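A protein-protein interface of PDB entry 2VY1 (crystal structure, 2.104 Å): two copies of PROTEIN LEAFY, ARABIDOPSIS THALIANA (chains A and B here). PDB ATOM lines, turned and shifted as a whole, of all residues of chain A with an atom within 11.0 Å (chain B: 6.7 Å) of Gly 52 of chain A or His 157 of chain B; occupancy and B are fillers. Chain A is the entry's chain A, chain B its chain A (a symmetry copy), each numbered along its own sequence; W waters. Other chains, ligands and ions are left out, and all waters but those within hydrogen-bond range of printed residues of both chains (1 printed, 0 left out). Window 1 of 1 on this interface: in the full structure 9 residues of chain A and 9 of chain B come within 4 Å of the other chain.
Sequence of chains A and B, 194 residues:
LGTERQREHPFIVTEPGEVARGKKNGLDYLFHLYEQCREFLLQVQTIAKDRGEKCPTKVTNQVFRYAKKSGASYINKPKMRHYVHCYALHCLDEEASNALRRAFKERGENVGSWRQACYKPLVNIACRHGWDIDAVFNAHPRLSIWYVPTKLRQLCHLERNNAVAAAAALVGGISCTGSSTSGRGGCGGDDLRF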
ATOM      1  N   VAL A  44      -0.526 -21.433  11.218  1.00  0.00           N
ATOM      2  CA  VAL A  44      -0.176 -22.745  11.766  1.00  0.00           C
ATOM      3  C   VAL A  44       0.905 -22.591  12.837  1.00  0.00           C
ATOM      4  O   VAL A  44       0.836 -23.213  13.893  1.00  0.00           O
ATOM      5  CB  VAL A  44       0.312 -23.709  10.653  1.00  0.00           C
ATOM      6  CG1 VAL A  44       1.023 -24.932  11.254  1.00  0.00           C
ATOM      7  CG2 VAL A  44      -0.859 -24.125   9.754  1.00  0.00           C
ATOM      8  N   GLN A  45       1.892 -21.742  12.562  1.00  0.00           N
ATOM      9  CA  GLN A  45       2.973 -21.485  13.513  1.00  0.00           C
ATOM     10  C   GLN A  45       2.456 -20.857  14.814  1.00  0.00           C
ATOM     11  O   GLN A  45       2.890 -21.218  15.905  1.00  0.00           O
ATOM     12  CB  GLN A  45       4.031 -20.578  12.888  1.00  0.00           C
ATOM     13  CG  GLN A  45       4.807 -21.234  11.734  1.00  0.00           C
ATOM     14  CD  GLN A  45       5.725 -20.255  11.046  1.00  0.00           C
ATOM     15  OE1 GLN A  45       5.412 -19.073  10.941  1.00  0.00           O
ATOM     16  NE2 GLN A  45       6.876 -20.738  10.585  1.00  0.00           N
ATOM     17  N   THR A  46       1.545 -19.903  14.686  1.00  0.00           N
ATOM     18  CA  THR A  46       0.966 -19.244  15.852  1.00  0.00           C
ATOM     19  C   THR A  46       0.332 -20.255  16.795  1.00  0.00           C
ATOM     20  O   THR A  46       0.551 -20.213  18.007  1.00  0.00           O
ATOM     21  CB  THR A  46      -0.058 -18.206  15.419  1.00  0.00           C
ATOM     22  OG1 THR A  46       0.634 -17.151  14.744  1.00  0.00           O
ATOM     23  CG2 THR A  46      -0.823 -17.632  16.630  1.00  0.00           C
ATOM     24  N   ILE A  47      -0.425 -21.184  16.225  1.00  0.00           N
ATOM     25  CA  ILE A  47      -1.141 -22.174  17.012  1.00  0.00           C
ATOM     26  C   ILE A  47      -0.205 -23.237  17.586  1.00  0.00           C
ATOM     27  O   ILE A  47      -0.347 -23.624  18.748  1.00  0.00           O
ATOM     28  CB  ILE A  47      -2.263 -22.841  16.195  1.00  0.00           C
ATOM     29  CG1 ILE A  47      -3.306 -21.797  15.789  1.00  0.00           C
ATOM     30  CG2 ILE A  47      -2.920 -23.942  16.996  1.00  0.00           C
ATOM     31  CD1 ILE A  47      -3.797 -20.924  16.955  1.00  0.00           C
ATOM     32  N   ALA A  48       0.748 -23.701  16.774  1.00  0.00           N
ATOM     33  CA  ALA A  48       1.747 -24.656  17.252  1.00  0.00           C
ATOM     34  C   ALA A  48       2.478 -24.097  18.468  1.00  0.00           C
ATOM     35  O   ALA A  48       2.642 -24.792  19.474  1.00  0.00           O
ATOM     36  CB  ALA A  48       2.758 -25.019  16.131  1.00  0.00           C
ATOM     37  N   LYS A  49       2.918 -22.844  18.380  1.00  0.00           N
ATOM     38  CA  LYS A  49       3.649 -22.219  19.487  1.00  0.00           C
ATOM     39  C   LYS A  49       2.766 -22.024  20.731  1.00  0.00           C
ATOM     40  O   LYS A  49       3.207 -22.233  21.860  1.00  0.00           O
ATOM     41  CB  LYS A  49       4.280 -20.890  19.057  1.00  0.00           C
ATOM     42  CG  LYS A  49       5.387 -21.044  18.017  1.00  0.00           C
ATOM     43  CD  LYS A  49       6.182 -19.759  17.830  1.00  0.00           C
ATOM     44  CE  LYS A  49       5.375 -18.700  17.107  1.00  0.00           C
ATOM     45  NZ  LYS A  49       6.217 -17.527  16.713  1.00  0.00           N
ATOM     46  N   ASP A  50       1.518 -21.626  20.527  1.00  0.00           N
ATOM     47  CA  ASP A  50       0.607 -21.461  21.656  1.00  0.00           C
ATOM     48  C   ASP A  50       0.318 -22.793  22.347  1.00  0.00           C
ATOM     49  O   ASP A  50       0.184 -22.851  23.569  1.00  0.00           O
ATOM     50  CB  ASP A  50      -0.705 -20.808  21.215  1.00  0.00           C
ATOM     51  CG  ASP A  50      -1.544 -20.345  22.398  1.00  0.00           C
ATOM     52  OD1 ASP A  50      -1.094 -19.428  23.119  1.00  0.00           O
ATOM     53  OD2 ASP A  50      -2.640 -20.902  22.600  1.00  0.00           O
ATOM     54  N   ARG A  51       0.210 -23.865  21.567  1.00  0.00           N
ATOM     55  CA  ARG A  51      -0.054 -25.183  22.134  1.00  0.00           C
ATOM     56  C   ARG A  51       1.207 -25.895  22.633  1.00  0.00           C
ATOM     57  O   ARG A  51       1.133 -27.014  23.136  1.00  0.00           O
ATOM     58  CB  ARG A  51      -0.766 -26.078  21.119  1.00  0.00           C
ATOM     59  CG  ARG A  51      -2.160 -25.620  20.724  1.00  0.00           C
ATOM     60  CD  ARG A  51      -2.677 -26.479  19.566  1.00  0.00           C
ATOM     61  NE  ARG A  51      -4.042 -26.126  19.198  1.00  0.00           N
ATOM     62  CZ  ARG A  51      -4.753 -26.747  18.261  1.00  0.00           C
ATOM     63  NH1 ARG A  51      -4.225 -27.759  17.580  1.00  0.00           N
ATOM     64  NH2 ARG A  51      -5.994 -26.351  18.005  1.00  0.00           N
ATOM     65  N   GLY A  52       2.363 -25.256  22.491  1.00  0.00           N
ATOM     66  CA  GLY A  52       3.606 -25.886  22.889  1.00  0.00           C
ATOM     67  C   GLY A  52       3.997 -27.060  22.002  1.00  0.00           C
ATOM     68  O   GLY A  52       4.679 -27.976  22.455  1.00  0.00           O
ATOM     69  N   GLU A  53       3.563 -27.038  20.743  1.00  0.00           N
ATOM     70  CA  GLU A  53       3.918 -28.095  19.795  1.00  0.00           C
ATOM     71  C   GLU A  53       5.123 -27.685  18.957  1.00  0.00           C
ATOM     72  O   GLU A  53       5.495 -26.509  18.910  1.00  0.00           O
ATOM     73  CB  GLU A  53       2.734 -28.436  18.877  1.00  0.00           C
ATOM     74  CG  GLU A  53       1.532 -29.032  19.607  1.00  0.00           C
ATOM     75  CD  GLU A  53       0.277 -29.069  18.751  1.00  0.00           C
ATOM     76  OE1 GLU A  53       0.269 -28.448  17.666  1.00  0.00           O
ATOM     77  OE2 GLU A  53      -0.712 -29.709  19.165  1.00  0.00           O
ATOM     78  N   LYS A  54       5.749 -28.652  18.299  1.00  0.00           N
ATOM     79  CA  LYS A  54       6.822 -28.307  17.375  1.00  0.00           C
ATOM     80  C   LYS A  54       6.262 -27.398  16.278  1.00  0.00           C
ATOM     81  O   LYS A  54       5.229 -27.690  15.678  1.00  0.00           O
ATOM     82  CB  LYS A  54       7.485 -29.556  16.795  1.00  0.00           C
ATOM     83  CG  LYS A  54       6.524 -30.583  16.209  1.00  0.00           C
ATOM     84  CD  LYS A  54       7.286 -31.826  15.764  1.00  0.00           C
ATOM     85  CE  LYS A  54       6.567 -32.571  14.652  1.00  0.00           C
ATOM     86  NZ  LYS A  54       7.419 -33.662  14.090  1.00  0.00           N
ATOM     87  N   CYS A  55       6.941 -26.282  16.055  1.00  0.00           N
ATOM     88  CA  CYS A  55       6.523 -25.278  15.092  1.00  0.00           C
ATOM     89  C   CYS A  55       7.215 -25.486  13.746  1.00  0.00           C
ATOM     90  O   CYS A  55       8.438 -25.408  13.662  1.00  0.00           O
ATOM     91  CB  CYS A  55       6.903 -23.906  15.632  1.00  0.00           C
ATOM     92  SG  CYS A  55       6.439 -22.508  14.611  1.00  0.00           S
ATOM     93  N   PRO A  56       6.435 -25.729  12.680  1.00  0.00           N
ATOM     94  CA  PRO A  56       7.031 -25.887  11.345  1.00  0.00           C
ATOM     95  C   PRO A  56       7.692 -24.591  10.870  1.00  0.00           C
ATOM     96  O   PRO A  56       7.212 -23.501  11.177  1.00  0.00           O
ATOM     97  CB  PRO A  56       5.817 -26.225  10.464  1.00  0.00           C
ATOM     98  CG  PRO A  56       4.645 -25.636  11.217  1.00  0.00           C
ATOM     99  CD  PRO A  56       4.974 -25.924  12.653  1.00  0.00           C
ATOM    100  N   GLN A  62       0.671 -30.020   6.542  1.00  0.00           N
ATOM    101  CA  GLN A  62      -0.180 -29.404   7.557  1.00  0.00           C
ATOM    102  C   GLN A  62      -0.719 -28.064   7.054  1.00  0.00           C
ATOM    103  O   GLN A  62      -1.899 -27.748   7.204  1.00  0.00           O
ATOM    104  CB  GLN A  62       0.622 -29.223   8.856  1.00  0.00           C
ATOM    105  CG  GLN A  62      -0.187 -28.747  10.050  1.00  0.00           C
ATOM    106  CD  GLN A  62       0.631 -28.705  11.334  1.00  0.00           C
ATOM    107  OE1 GLN A  62       1.831 -28.992  11.339  1.00  0.00           O
ATOM    108  NE2 GLN A  62      -0.018 -28.336  12.430  1.00  0.00           N
ATOM    109  N   TRP B 131      11.174 -20.415  28.404  1.00  0.00           N
ATOM    110  CA  TRP B 131      10.472 -21.663  28.116  1.00  0.00           C
ATOM    111  C   TRP B 131      10.663 -22.154  26.677  1.00  0.00           C
ATOM    112  O   TRP B 131       9.898 -22.985  26.190  1.00  0.00           O
ATOM    113  CB  TRP B 131       8.985 -21.514  28.425  1.00  0.00           C
ATOM    114  CG  TRP B 131       8.723 -21.159  29.855  1.00  0.00           C
ATOM    115  CD1 TRP B 131       8.408 -19.926  30.352  1.00  0.00           C
ATOM    116  CD2 TRP B 131       8.772 -22.046  30.979  1.00  0.00           C
ATOM    117  NE1 TRP B 131       8.251 -19.993  31.717  1.00  0.00           N
ATOM    118  CE2 TRP B 131       8.468 -21.283  32.126  1.00  0.00           C
ATOM    119  CE3 TRP B 131       9.041 -23.410  31.129  1.00  0.00           C
ATOM    120  CZ2 TRP B 131       8.422 -21.840  33.403  1.00  0.00           C
ATOM    121  CZ3 TRP B 131       8.995 -23.962  32.397  1.00  0.00           C
ATOM    122  CH2 TRP B 131       8.687 -23.177  33.518  1.00  0.00           C
ATOM    123  N   LEU B 152       9.355 -34.186  27.144  1.00  0.00           N
ATOM    124  CA  LEU B 152      10.053 -32.990  27.612  1.00  0.00           C
ATOM    125  C   LEU B 152       9.350 -31.711  27.146  1.00  0.00           C
ATOM    126  O   LEU B 152       9.203 -30.745  27.908  1.00  0.00           O
ATOM    127  CB  LEU B 152      11.506 -32.993  27.141  1.00  0.00           C
ATOM    128  CG  LEU B 152      12.314 -31.746  27.490  1.00  0.00           C
ATOM    129  CD1 LEU B 152      12.312 -31.493  29.001  1.00  0.00           C
ATOM    130  CD2 LEU B 152      13.728 -31.879  26.962  1.00  0.00           C
ATOM    131  N   ARG B 153       8.921 -31.707  25.887  1.00  0.00           N
ATOM    132  CA  ARG B 153       8.200 -30.563  25.344  1.00  0.00           C
ATOM    133  C   ARG B 153       6.886 -30.344  26.105  1.00  0.00           C
ATOM    134  O   ARG B 153       6.562 -29.221  26.484  1.00  0.00           O
ATOM    135  CB  ARG B 153       7.932 -30.765  23.851  1.00  0.00           C
ATOM    136  CG  ARG B 153       7.522 -29.504  23.115  1.00  0.00           C
ATOM    137  CD  ARG B 153       7.123 -29.815  21.668  1.00  0.00           C
ATOM    138  NE  ARG B 153       8.264 -30.155  20.816  1.00  0.00           N
ATOM    139  CZ  ARG B 153       9.140 -29.265  20.360  1.00  0.00           C
ATOM    140  NH1 ARG B 153       9.016 -27.986  20.689  1.00  0.00           N
ATOM    141  NH2 ARG B 153      10.144 -29.649  19.580  1.00  0.00           N
ATOM    142  N   GLN B 154       6.139 -31.419  26.335  1.00  0.00           N
ATOM    143  CA  GLN B 154       4.878 -31.323  27.071  1.00  0.00           C
ATOM    144  C   GLN B 154       5.065 -30.767  28.486  1.00  0.00           C
ATOM    145  O   GLN B 154       4.302 -29.910  28.925  1.00  0.00           O
ATOM    146  CB  GLN B 154       4.180 -32.681  27.123  1.00  0.00           C
ATOM    147  CG  GLN B 154       3.565 -33.098  25.807  1.00  0.00           C
ATOM    148  CD  GLN B 154       3.222 -34.576  25.768  1.00  0.00           C
ATOM    149  OE1 GLN B 154       3.626 -35.342  26.646  1.00  0.00           O
ATOM    150  NE2 GLN B 154       2.481 -34.985  24.744  1.00  0.00           N
ATOM    151  N   LEU B 155       6.086 -31.251  29.191  1.00  0.00           N
ATOM    152  CA  LEU B 155       6.369 -30.784  30.546  1.00  0.00           C
ATOM    153  C   LEU B 155       6.739 -29.310  30.569  1.00  0.00           C
ATOM    154  O   LEU B 155       6.324 -28.576  31.467  1.00  0.00           O
ATOM    155  CB  LEU B 155       7.492 -31.600  31.191  1.00  0.00           C
ATOM    156  CG  LEU B 155       7.171 -33.050  31.544  1.00  0.00           C
ATOM    157  CD1 LEU B 155       8.451 -33.806  31.862  1.00  0.00           C
ATOM    158  CD2 LEU B 155       6.180 -33.120  32.717  1.00  0.00           C
ATOM    159  N   CYS B 156       7.534 -28.878  29.594  1.00  0.00           N
ATOM    160  CA  CYS B 156       7.936 -27.478  29.515  1.00  0.00           C
ATOM    161  C   CYS B 156       6.720 -26.590  29.284  1.00  0.00           C
ATOM    162  O   CYS B 156       6.646 -25.474  29.807  1.00  0.00           O
ATOM    163  CB  CYS B 156       8.968 -27.255  28.404  1.00  0.00           C
ATOM    164  SG  CYS B 156      10.623 -27.863  28.794  1.00  0.00           S
ATOM    165  N   HIS B 157       5.770 -27.090  28.501  1.00  0.00           N
ATOM    166  CA  HIS B 157       4.565 -26.330  28.198  1.00  0.00           C
ATOM    167  C   HIS B 157       3.624 -26.293  29.399  1.00  0.00           C
ATOM    168  O   HIS B 157       3.045 -25.256  29.708  1.00  0.00           O
ATOM    169  CB  HIS B 157       3.840 -26.912  26.986  1.00  0.00           C
ATOM    170  CG  HIS B 157       2.669 -26.095  26.537  1.00  0.00           C
ATOM    171  ND1 HIS B 157       1.377 -26.582  26.530  1.00  0.00           N
ATOM    172  CD2 HIS B 157       2.589 -24.819  26.092  1.00  0.00           C
ATOM    173  CE1 HIS B 157       0.557 -25.644  26.092  1.00  0.00           C
ATOM    174  NE2 HIS B 157       1.267 -24.563  25.818  1.00  0.00           N
ATOM    175  N   LEU B 158       3.469 -27.440  30.052  1.00  0.00           N
ATOM    176  CA  LEU B 158       2.673 -27.550  31.270  1.00  0.00           C
ATOM    177  C   LEU B 158       3.192 -26.598  32.329  1.00  0.00           C
ATOM    178  O   LEU B 158       2.419 -25.972  33.051  1.00  0.00           O
ATOM    179  CB  LEU B 158       2.718 -28.983  31.804  1.00  0.00           C
ATOM    180  CG  LEU B 158       1.479 -29.858  31.616  1.00  0.00           C
ATOM    181  CD1 LEU B 158       1.856 -31.302  31.305  1.00  0.00           C
ATOM    182  CD2 LEU B 158       0.588 -29.782  32.856  1.00  0.00           C
ATOM    183  N   GLU B 159       4.512 -26.488  32.408  1.00  0.00           N
ATOM    184  CA  GLU B 159       5.144 -25.666  33.428  1.00  0.00           C
ATOM    185  C   GLU B 159       5.047 -24.177  33.108  1.00  0.00           C
ATOM    186  O   GLU B 159       4.826 -23.360  34.002  1.00  0.00           O
ATOM    187  CB  GLU B 159       6.604 -26.081  33.625  1.00  0.00           C
ATOM    188  CG  GLU B 159       7.131 -25.779  35.014  1.00  0.00           C
ATOM    189  CD  GLU B 159       6.144 -26.171  36.100  1.00  0.00           C
ATOM    190  OE1 GLU B 159       5.889 -27.383  36.274  1.00  0.00           O
ATOM    191  OE2 GLU B 159       5.618 -25.261  36.775  1.00  0.00           O
ATOM    192  N   ARG B 160       5.215 -23.824  31.837  1.00  0.00           N
ATOM    193  CA  ARG B 160       5.073 -22.433  31.424  1.00  0.00           C
ATOM    194  C   ARG B 160       3.658 -21.924  31.682  1.00  0.00           C
ATOM    195  O   ARG B 160       3.464 -20.772  32.064  1.00  0.00           O
ATOM    196  CB  ARG B 160       5.440 -22.251  29.951  1.00  0.00           C
ATOM    197  CG  ARG B 160       4.659 -21.146  29.258  1.00  0.00           C
ATOM    198  CD  ARG B 160       5.406 -20.607  28.050  1.00  0.00           C
ATOM    199  NE  ARG B 160       4.505 -20.304  26.940  1.00  0.00           N
ATOM    200  CZ  ARG B 160       4.473 -20.984  25.796  1.00  0.00           C
ATOM    201  NH1 ARG B 160       5.301 -22.005  25.604  1.00  0.00           N
ATOM    202  NH2 ARG B 160       3.618 -20.641  24.837  1.00  0.00           N
ATOM    203  N   ASN B 161       2.671 -22.785  31.468  1.00  0.00           N
ATOM    204  CA  ASN B 161       1.288 -22.415  31.724  1.00  0.00           C
ATOM    205  C   ASN B 161       1.051 -22.201  33.218  1.00  0.00           C
ATOM    206  O   ASN B 161       0.452 -21.206  33.624  1.00  0.00           O
ATOM    207  CB  ASN B 161       0.327 -23.463  31.157  1.00  0.00           C
ATOM    208  CG  ASN B 161       0.087 -23.288  29.662  1.00  0.00           C
ATOM    209  OD1 ASN B 161       0.517 -22.300  29.059  1.00  0.00           O
ATOM    210  ND2 ASN B 161      -0.607 -24.247  29.060  1.00  0.00           N
ATOM    211  N   ASN B 162       1.529 -23.138  34.033  1.00  0.00           N
ATOM    212  CA  ASN B 162       1.459 -22.983  35.480  1.00  0.00           C
ATOM    213  C   ASN B 162       2.154 -21.703  35.918  1.00  0.00           C
ATOM    214  O   ASN B 162       1.736 -21.056  36.875  1.00  0.00           O
ATOM    215  CB  ASN B 162       2.073 -24.192  36.187  1.00  0.00           C
ATOM    216  CG  ASN B 162       1.207 -25.430  36.075  1.00  0.00           C
ATOM    217  OD1 ASN B 162       0.051 -25.357  35.656  1.00  0.00           O
ATOM    218  ND2 ASN B 162       1.762 -26.578  36.450  1.00  0.00           N
HETATM  219  O   HOH W   1       7.321 -26.383  22.446  1.00  0.00           O
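Water W1 lies within hydrogen-bond range of NH1 of Arg 153 of chain B (2.9 Å) and O of Gly 52 of chain A (3.1 Å).
Of the 14 printed residues of chain A, 6 touch a printed residue of chain B. Printed residues of chain A that touch a printed residue of chain B: Lys 49, Asp 50, Arg 51, Gly 52, Glu 53 and Lys 54. Printed residues of chain B that touch a printed residue of chain A: Arg 153, His 157 and Arg 160. Hydrophobic or aromatic side chains of chain B that line the printed part of chain A: His 157. Among the printed residues, 7 pairs touch across the chains. Among the printed residues, no Asp or Glu carboxylate lies within 4 Å of a Lys or Arg side-chain nitrogen of the other chain.
O of Lys 49 of chain A lies within hydrogen-bond range of NH2 of Arg 160 of chain B, at 3.4 Å. O of Asp 50 of chain A lies within hydrogen-bond range of NE2 of His 157 of chain B. The backbone carbonyl oxygen of Arg 51 of chain A sits close to a ring nitrogen (ND1) of His 157 of chain B, at 3.4 Å.
No position is printed for both chains. Of the 7 pairs that touch across the chains among the printed residues, none has its exchanged pair printed and touching as well.
Of the printed residues of chain B, Lys 49 of chain A touches Arg 160 (3.4 Å). Of the printed residues of chain B, Arg 51 of chain A touches His 157 (3.3 Å). Of chain B, only Arg 153 (3.2 Å) and His 157 (3.5 Å) come within 4 Å of Gly 52 of chain A. Of the printed residues of chain B, Glu 53 of chain A touches Arg 153. Of the printed residues of chain A, Arg 153 of chain B touches Gly 52, Glu 53 and Lys 54. Leu 155 of chain B touches none of the printed residues of chain A. Cys 156 of chain B touches none of the printed residues of chain A. Of the printed residues of chain A, His 157 of chain B touches Asp 50 (3.0 Å), Arg 51 (3.3 Å) and Gly 52 (3.5 Å). Glu 159 of chain B touches none of the printed residues of chain A. No residue of chain A comes within 4 Å of Asn 161 of chain B. The nearest residue of chain A that does not touch His 157 of chain B is Lys 49 of chain A (5.0 Å).
Gly 52 of chain A touches Arg 153 of chain B. Gly 52 of chain A touches His 157 of chain B (CA to CD2, 3.5 Å). Arg 153 of chain B touches Glu 53 of chain A. Arg 153 of chain B touches Lys 54 of chain A (CD to N, 3.8 Å).
O of Ala 48 of chain A sits at hydrogen-bond distance from N of Glu 53 of chain A (2.7 Å).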
